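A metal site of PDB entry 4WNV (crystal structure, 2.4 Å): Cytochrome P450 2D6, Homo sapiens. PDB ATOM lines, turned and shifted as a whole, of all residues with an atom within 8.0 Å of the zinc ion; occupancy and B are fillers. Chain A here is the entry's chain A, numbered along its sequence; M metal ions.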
ATOM      1  N   TRP A 130      -8.977   2.153 -20.729  1.00  0.00           N
ATOM      2  CA  TRP A 130      -8.474   2.663 -22.002  1.00  0.00           C
ATOM      3  C   TRP A 130      -8.022   1.546 -22.927  1.00  0.00           C
ATOM      4  O   TRP A 130      -8.308   1.566 -24.120  1.00  0.00           O
ATOM      5  CB  TRP A 130      -7.309   3.635 -21.789  1.00  0.00           C
ATOM      6  CG  TRP A 130      -7.719   5.008 -21.375  1.00  0.00           C
ATOM      7  CD1 TRP A 130      -8.785   5.718 -21.821  1.00  0.00           C
ATOM      8  CD2 TRP A 130      -7.054   5.831 -20.417  1.00  0.00           C
ATOM      9  NE1 TRP A 130      -8.835   6.949 -21.202  1.00  0.00           N
ATOM     10  CE2 TRP A 130      -7.776   7.041 -20.335  1.00  0.00           C
ATOM     11  CE3 TRP A 130      -5.903   5.678 -19.615  1.00  0.00           C
ATOM     12  CZ2 TRP A 130      -7.402   8.092 -19.482  1.00  0.00           C
ATOM     13  CZ3 TRP A 130      -5.537   6.730 -18.770  1.00  0.00           C
ATOM     14  CH2 TRP A 130      -6.268   7.913 -18.711  1.00  0.00           C
ATOM     15  N   ALA A 165      -1.223   7.469 -25.983  1.00  0.00           N
ATOM     16  CA  ALA A 165      -1.961   8.719 -26.081  1.00  0.00           C
ATOM     17  C   ALA A 165      -2.927   8.865 -24.900  1.00  0.00           C
ATOM     18  O   ALA A 165      -3.079   9.952 -24.353  1.00  0.00           O
ATOM     19  CB  ALA A 165      -2.720   8.794 -27.403  1.00  0.00           C
ATOM     20  N   SER A 166      -3.580   7.776 -24.518  1.00  0.00           N
ATOM     21  CA  SER A 166      -4.483   7.818 -23.385  1.00  0.00           C
ATOM     22  C   SER A 166      -3.726   8.087 -22.089  1.00  0.00           C
ATOM     23  O   SER A 166      -4.093   8.942 -21.311  1.00  0.00           O
ATOM     24  CB  SER A 166      -5.285   6.521 -23.277  1.00  0.00           C
ATOM     25  OG  SER A 166      -6.079   6.342 -24.438  1.00  0.00           O
ATOM     26  N   LEU A 167      -2.674   7.308 -21.851  1.00  0.00           N
ATOM     27  CA  LEU A 167      -1.803   7.489 -20.696  1.00  0.00           C
ATOM     28  C   LEU A 167      -1.305   8.926 -20.607  1.00  0.00           C
ATOM     29  O   LEU A 167      -1.348   9.547 -19.543  1.00  0.00           O
ATOM     30  CB  LEU A 167      -0.608   6.520 -20.783  1.00  0.00           C
ATOM     31  CG  LEU A 167       0.702   6.835 -20.042  1.00  0.00           C
ATOM     32  CD1 LEU A 167       0.463   6.885 -18.566  1.00  0.00           C
ATOM     33  CD2 LEU A 167       1.798   5.802 -20.351  1.00  0.00           C
ATOM     34  N   THR A 168      -0.803   9.463 -21.719  1.00  0.00           N
ATOM     35  CA  THR A 168      -0.090  10.727 -21.697  1.00  0.00           C
ATOM     36  C   THR A 168      -1.009  11.940 -21.816  1.00  0.00           C
ATOM     37  O   THR A 168      -0.872  12.882 -21.052  1.00  0.00           O
ATOM     38  CB  THR A 168       0.976  10.790 -22.811  1.00  0.00           C
ATOM     39  OG1 THR A 168       0.369  10.548 -24.097  1.00  0.00           O
ATOM     40  CG2 THR A 168       2.091   9.751 -22.555  1.00  0.00           C
ATOM     41  N   CYS A 169      -1.973  11.916 -22.743  1.00  0.00           N
ATOM     42  CA  CYS A 169      -2.821  13.086 -22.982  1.00  0.00           C
ATOM     43  C   CYS A 169      -4.304  12.854 -22.667  1.00  0.00           C
ATOM     44  O   CYS A 169      -5.117  13.748 -22.861  1.00  0.00           O
ATOM     45  CB  CYS A 169      -2.666  13.544 -24.424  1.00  0.00           C
ATOM     46  SG  CYS A 169      -0.960  13.920 -24.946  1.00  0.00           S
ATOM     47  N   GLY A 170      -4.659  11.673 -22.169  1.00  0.00           N
ATOM     48  CA  GLY A 170      -6.042  11.385 -21.805  1.00  0.00           C
ATOM     49  C   GLY A 170      -7.016  11.375 -22.992  1.00  0.00           C
ATOM     50  O   GLY A 170      -8.216  11.682 -22.839  1.00  0.00           O
ATOM     51  N   ARG A 171      -6.522  11.030 -24.177  1.00  0.00           N
ATOM     52  CA  ARG A 171      -7.389  10.892 -25.316  1.00  0.00           C
ATOM     53  C   ARG A 171      -6.895   9.804 -26.237  1.00  0.00           C
ATOM     54  O   ARG A 171      -5.746   9.391 -26.152  1.00  0.00           O
ATOM     55  CB  ARG A 171      -7.462  12.187 -26.110  1.00  0.00           C
ATOM     56  CG  ARG A 171      -6.169  12.486 -26.809  1.00  0.00           C
ATOM     57  CD  ARG A 171      -6.370  13.558 -27.815  1.00  0.00           C
ATOM     58  NE  ARG A 171      -7.259  13.096 -28.857  1.00  0.00           N
ATOM     59  CZ  ARG A 171      -7.632  13.837 -29.888  1.00  0.00           C
ATOM     60  NH1 ARG A 171      -7.195  15.089 -30.002  1.00  0.00           N
ATOM     61  NH2 ARG A 171      -8.452  13.333 -30.806  1.00  0.00           N
ATOM     62  N   HIS A 236      -3.492  20.174 -25.304  1.00  0.00           N
ATOM     63  CA  HIS A 236      -3.873  19.507 -24.073  1.00  0.00           C
ATOM     64  C   HIS A 236      -3.777  20.476 -22.908  1.00  0.00           C
ATOM     65  O   HIS A 236      -4.525  20.380 -21.948  1.00  0.00           O
ATOM     66  CB  HIS A 236      -2.998  18.276 -23.855  1.00  0.00           C
ATOM     67  CG  HIS A 236      -3.406  17.461 -22.673  1.00  0.00           C
ATOM     68  ND1 HIS A 236      -2.508  16.701 -21.963  1.00  0.00           N
ATOM     69  CD2 HIS A 236      -4.603  17.281 -22.070  1.00  0.00           C
ATOM     70  CE1 HIS A 236      -3.131  16.071 -20.982  1.00  0.00           C
ATOM     71  NE2 HIS A 236      -4.403  16.411 -21.024  1.00  0.00           N
ATOM     72  N   ARG A 237      -2.858  21.418 -23.006  1.00  0.00           N
ATOM     73  CA  ARG A 237      -2.632  22.384 -21.944  1.00  0.00           C
ATOM     74  C   ARG A 237      -3.809  23.346 -21.789  1.00  0.00           C
ATOM     75  O   ARG A 237      -4.082  23.839 -20.695  1.00  0.00           O
ATOM     76  CB  ARG A 237      -1.356  23.150 -22.240  1.00  0.00           C
ATOM     77  CG  ARG A 237      -0.589  23.571 -21.021  1.00  0.00           C
ATOM     78  CD  ARG A 237       0.866  23.756 -21.385  1.00  0.00           C
ATOM     79  NE  ARG A 237       1.623  24.382 -20.302  1.00  0.00           N
ATOM     80  CZ  ARG A 237       2.943  24.309 -20.204  1.00  0.00           C
ATOM     81  NH1 ARG A 237       3.633  23.634 -21.129  1.00  0.00           N
ATOM     82  NH2 ARG A 237       3.574  24.889 -19.185  1.00  0.00           N
ATOM     83  N   THR A 239      -7.007  22.486 -22.331  1.00  0.00           N
ATOM     84  CA  THR A 239      -8.178  21.790 -21.818  1.00  0.00           C
ATOM     85  C   THR A 239      -7.988  21.278 -20.390  1.00  0.00           C
ATOM     86  O   THR A 239      -8.950  20.876 -19.738  1.00  0.00           O
ATOM     87  CB  THR A 239      -8.562  20.604 -22.705  1.00  0.00           C
ATOM     88  OG1 THR A 239      -7.442  19.738 -22.833  1.00  0.00           O
ATOM     89  CG2 THR A 239      -8.967  21.073 -24.065  1.00  0.00           C
ATOM     90  N   TRP A 240      -6.738  21.293 -19.909  1.00  0.00           N
ATOM     91  CA  TRP A 240      -6.403  20.797 -18.583  1.00  0.00           C
ATOM     92  C   TRP A 240      -7.183  21.548 -17.500  1.00  0.00           C
ATOM     93  O   TRP A 240      -7.209  22.778 -17.463  1.00  0.00           O
ATOM     94  CB  TRP A 240      -4.898  20.930 -18.304  1.00  0.00           C
ATOM     95  CG  TRP A 240      -4.454  20.629 -16.877  1.00  0.00           C
ATOM     96  CD1 TRP A 240      -4.910  19.631 -16.054  1.00  0.00           C
ATOM     97  CD2 TRP A 240      -3.453  21.328 -16.118  1.00  0.00           C
ATOM     98  NE1 TRP A 240      -4.253  19.676 -14.843  1.00  0.00           N
ATOM     99  CE2 TRP A 240      -3.347  20.702 -14.860  1.00  0.00           C
ATOM    100  CE3 TRP A 240      -2.625  22.422 -16.391  1.00  0.00           C
ATOM    101  CZ2 TRP A 240      -2.482  21.144 -13.867  1.00  0.00           C
ATOM    102  CZ3 TRP A 240      -1.746  22.869 -15.396  1.00  0.00           C
ATOM    103  CH2 TRP A 240      -1.683  22.220 -14.156  1.00  0.00           C
ATOM    104  N   ASP A 241      -7.812  20.773 -16.617  1.00  0.00           N
ATOM    105  CA  ASP A 241      -8.518  21.342 -15.490  1.00  0.00           C
ATOM    106  C   ASP A 241      -7.722  21.089 -14.199  1.00  0.00           C
ATOM    107  O   ASP A 241      -7.882  20.046 -13.567  1.00  0.00           O
ATOM    108  CB  ASP A 241      -9.915  20.754 -15.392  1.00  0.00           C
ATOM    109  CG  ASP A 241     -10.790  21.473 -14.417  1.00  0.00           C
ATOM    110  OD1 ASP A 241     -11.991  21.160 -14.369  1.00  0.00           O
ATOM    111  OD2 ASP A 241     -10.283  22.370 -13.704  1.00  0.00           O
ATOM    112  N   PRO A 245      -8.421  16.328 -10.086  1.00  0.00           N
ATOM    113  CA  PRO A 245      -7.260  15.433 -10.030  1.00  0.00           C
ATOM    114  C   PRO A 245      -6.763  15.131 -11.428  1.00  0.00           C
ATOM    115  O   PRO A 245      -7.593  14.994 -12.333  1.00  0.00           O
ATOM    116  CB  PRO A 245      -7.808  14.158  -9.363  1.00  0.00           C
ATOM    117  CG  PRO A 245      -8.969  14.630  -8.558  1.00  0.00           C
ATOM    118  CD  PRO A 245      -9.571  15.772  -9.349  1.00  0.00           C
ATOM    119  N   PRO A 246      -5.433  15.069 -11.610  1.00  0.00           N
ATOM    120  CA  PRO A 246      -4.821  14.730 -12.900  1.00  0.00           C
ATOM    121  C   PRO A 246      -5.459  13.505 -13.549  1.00  0.00           C
ATOM    122  O   PRO A 246      -5.582  12.479 -12.895  1.00  0.00           O
ATOM    123  CB  PRO A 246      -3.369  14.467 -12.530  1.00  0.00           C
ATOM    124  CG  PRO A 246      -3.134  15.307 -11.336  1.00  0.00           C
ATOM    125  CD  PRO A 246      -4.432  15.390 -10.583  1.00  0.00           C
ATOM    126  N   ARG A 247      -5.881  13.637 -14.804  1.00  0.00           N
ATOM    127  CA  ARG A 247      -6.510  12.536 -15.548  1.00  0.00           C
ATOM    128  C   ARG A 247      -5.469  11.631 -16.171  1.00  0.00           C
ATOM    129  O   ARG A 247      -5.734  10.467 -16.462  1.00  0.00           O
ATOM    130  CB  ARG A 247      -7.426  13.086 -16.652  1.00  0.00           C
ATOM    131  CG  ARG A 247      -8.797  13.515 -16.210  1.00  0.00           C
ATOM    132  CD  ARG A 247      -9.576  14.222 -17.320  1.00  0.00           C
ATOM    133  NE  ARG A 247      -8.949  15.494 -17.710  1.00  0.00           N
ATOM    134  CZ  ARG A 247      -9.602  16.633 -17.935  1.00  0.00           C
ATOM    135  NH1 ARG A 247     -10.933  16.695 -17.795  1.00  0.00           N
ATOM    136  NH2 ARG A 247      -8.921  17.734 -18.273  1.00  0.00           N
ATOM    137  N   ASP A 248      -4.294  12.185 -16.406  1.00  0.00           N
ATOM    138  CA  ASP A 248      -3.290  11.536 -17.231  1.00  0.00           C
ATOM    139  C   ASP A 248      -1.906  12.029 -16.828  1.00  0.00           C
ATOM    140  O   ASP A 248      -1.776  12.875 -15.955  1.00  0.00           O
ATOM    141  CB  ASP A 248      -3.547  11.814 -18.721  1.00  0.00           C
ATOM    142  CG  ASP A 248      -3.829  13.288 -18.995  1.00  0.00           C
ATOM    143  OD1 ASP A 248      -2.921  14.105 -18.813  1.00  0.00           O
ATOM    144  OD2 ASP A 248      -4.956  13.614 -19.399  1.00  0.00           O
ATOM    145  N   LEU A 249      -0.881  11.504 -17.487  1.00  0.00           N
ATOM    146  CA  LEU A 249       0.477  11.694 -17.024  1.00  0.00           C
ATOM    147  C   LEU A 249       0.946  13.139 -17.261  1.00  0.00           C
ATOM    148  O   LEU A 249       1.655  13.721 -16.435  1.00  0.00           O
ATOM    149  CB  LEU A 249       1.416  10.696 -17.699  1.00  0.00           C
ATOM    150  CG  LEU A 249       2.879  10.769 -17.271  1.00  0.00           C
ATOM    151  CD1 LEU A 249       3.522   9.391 -17.350  1.00  0.00           C
ATOM    152  CD2 LEU A 249       3.649  11.759 -18.126  1.00  0.00           C
ATOM    153  N   THR A 250       0.570  13.697 -18.411  1.00  0.00           N
ATOM    154  CA  THR A 250       0.878  15.091 -18.735  1.00  0.00           C
ATOM    155  C   THR A 250       0.320  16.065 -17.678  1.00  0.00           C
ATOM    156  O   THR A 250       0.926  17.083 -17.378  1.00  0.00           O
ATOM    157  CB  THR A 250       0.329  15.460 -20.147  1.00  0.00           C
ATOM    158  OG1 THR A 250       1.091  14.764 -21.147  1.00  0.00           O
ATOM    159  CG2 THR A 250       0.395  16.944 -20.414  1.00  0.00           C
ATOM    160  N   GLU A 251      -0.832  15.741 -17.095  1.00  0.00           N
ATOM    161  CA  GLU A 251      -1.467  16.651 -16.140  1.00  0.00           C
ATOM    162  C   GLU A 251      -0.815  16.508 -14.789  1.00  0.00           C
ATOM    163  O   GLU A 251      -0.588  17.505 -14.109  1.00  0.00           O
ATOM    164  CB  GLU A 251      -2.981  16.396 -16.038  1.00  0.00           C
ATOM    165  CG  GLU A 251      -3.739  16.672 -17.337  1.00  0.00           C
ATOM    166  CD  GLU A 251      -5.241  16.460 -17.172  1.00  0.00           C
ATOM    167  OE1 GLU A 251      -5.682  16.222 -16.027  1.00  0.00           O
ATOM    168  OE2 GLU A 251      -5.968  16.525 -18.184  1.00  0.00           O
ATOM    169  N   ALA A 252      -0.465  15.277 -14.425  1.00  0.00           N
ATOM    170  CA  ALA A 252       0.344  15.047 -13.244  1.00  0.00           C
ATOM    171  C   ALA A 252       1.653  15.827 -13.372  1.00  0.00           C
ATOM    172  O   ALA A 252       2.065  16.503 -12.434  1.00  0.00           O
ATOM    173  CB  ALA A 252       0.605  13.546 -13.025  1.00  0.00           C
ATOM    174  N   LEU A 254       2.267  18.439 -15.310  1.00  0.00           N
ATOM    175  CA  LEU A 254       1.981  19.872 -15.313  1.00  0.00           C
ATOM    176  C   LEU A 254       1.788  20.385 -13.898  1.00  0.00           C
ATOM    177  O   LEU A 254       2.270  21.467 -13.551  1.00  0.00           O
ATOM    178  CB  LEU A 254       0.751  20.186 -16.172  1.00  0.00           C
ATOM    179  CG  LEU A 254       0.994  20.141 -17.694  1.00  0.00           C
ATOM    180  CD1 LEU A 254      -0.326  20.300 -18.453  1.00  0.00           C
ATOM    181  CD2 LEU A 254       1.988  21.196 -18.127  1.00  0.00           C
HETATM  182 ZN    ZN M   1      -5.551  15.534 -19.800  1.00  0.00          ZN
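OD2 of Asp 248 lies close to N of Gly 170, at 3.4 Å. The backbone carbonyl oxygen (O) of Thr 239 is in hydrogen-bond range of the guanidinium group (NH2) of Arg 247 (3.5 Å). The guanidinium group (NE) of Arg 247 lies within salt-bridge range of the side-chain carboxylate (OE1) of Glu 251 (3.7 Å). SG of Cys 169 lies close to OG1 of Thr 168, at 3.7 Å. The backbone carbonyl oxygen (O) of Cys 169 sits close to a ring nitrogen (NE2) of His 236. O of His 236 sits at hydrogen-bond distance from OG1 of Thr 239 (3.1 Å).
NE2 of His 236 is bound to the zinc ion (1.9 Å). The zinc ion is bound by the side-chain carboxylate (OE2) of Glu 251 (1.9 Å). The zinc ion is bound by OD2 of Asp 248 (2.0 Å).
Cys 169 touches the zinc ion. NE of Arg 247 touches the zinc ion, at 3.99 Å. The nearest printed residue that does not touch the zinc ion is Gly 170 (4.6 Å).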
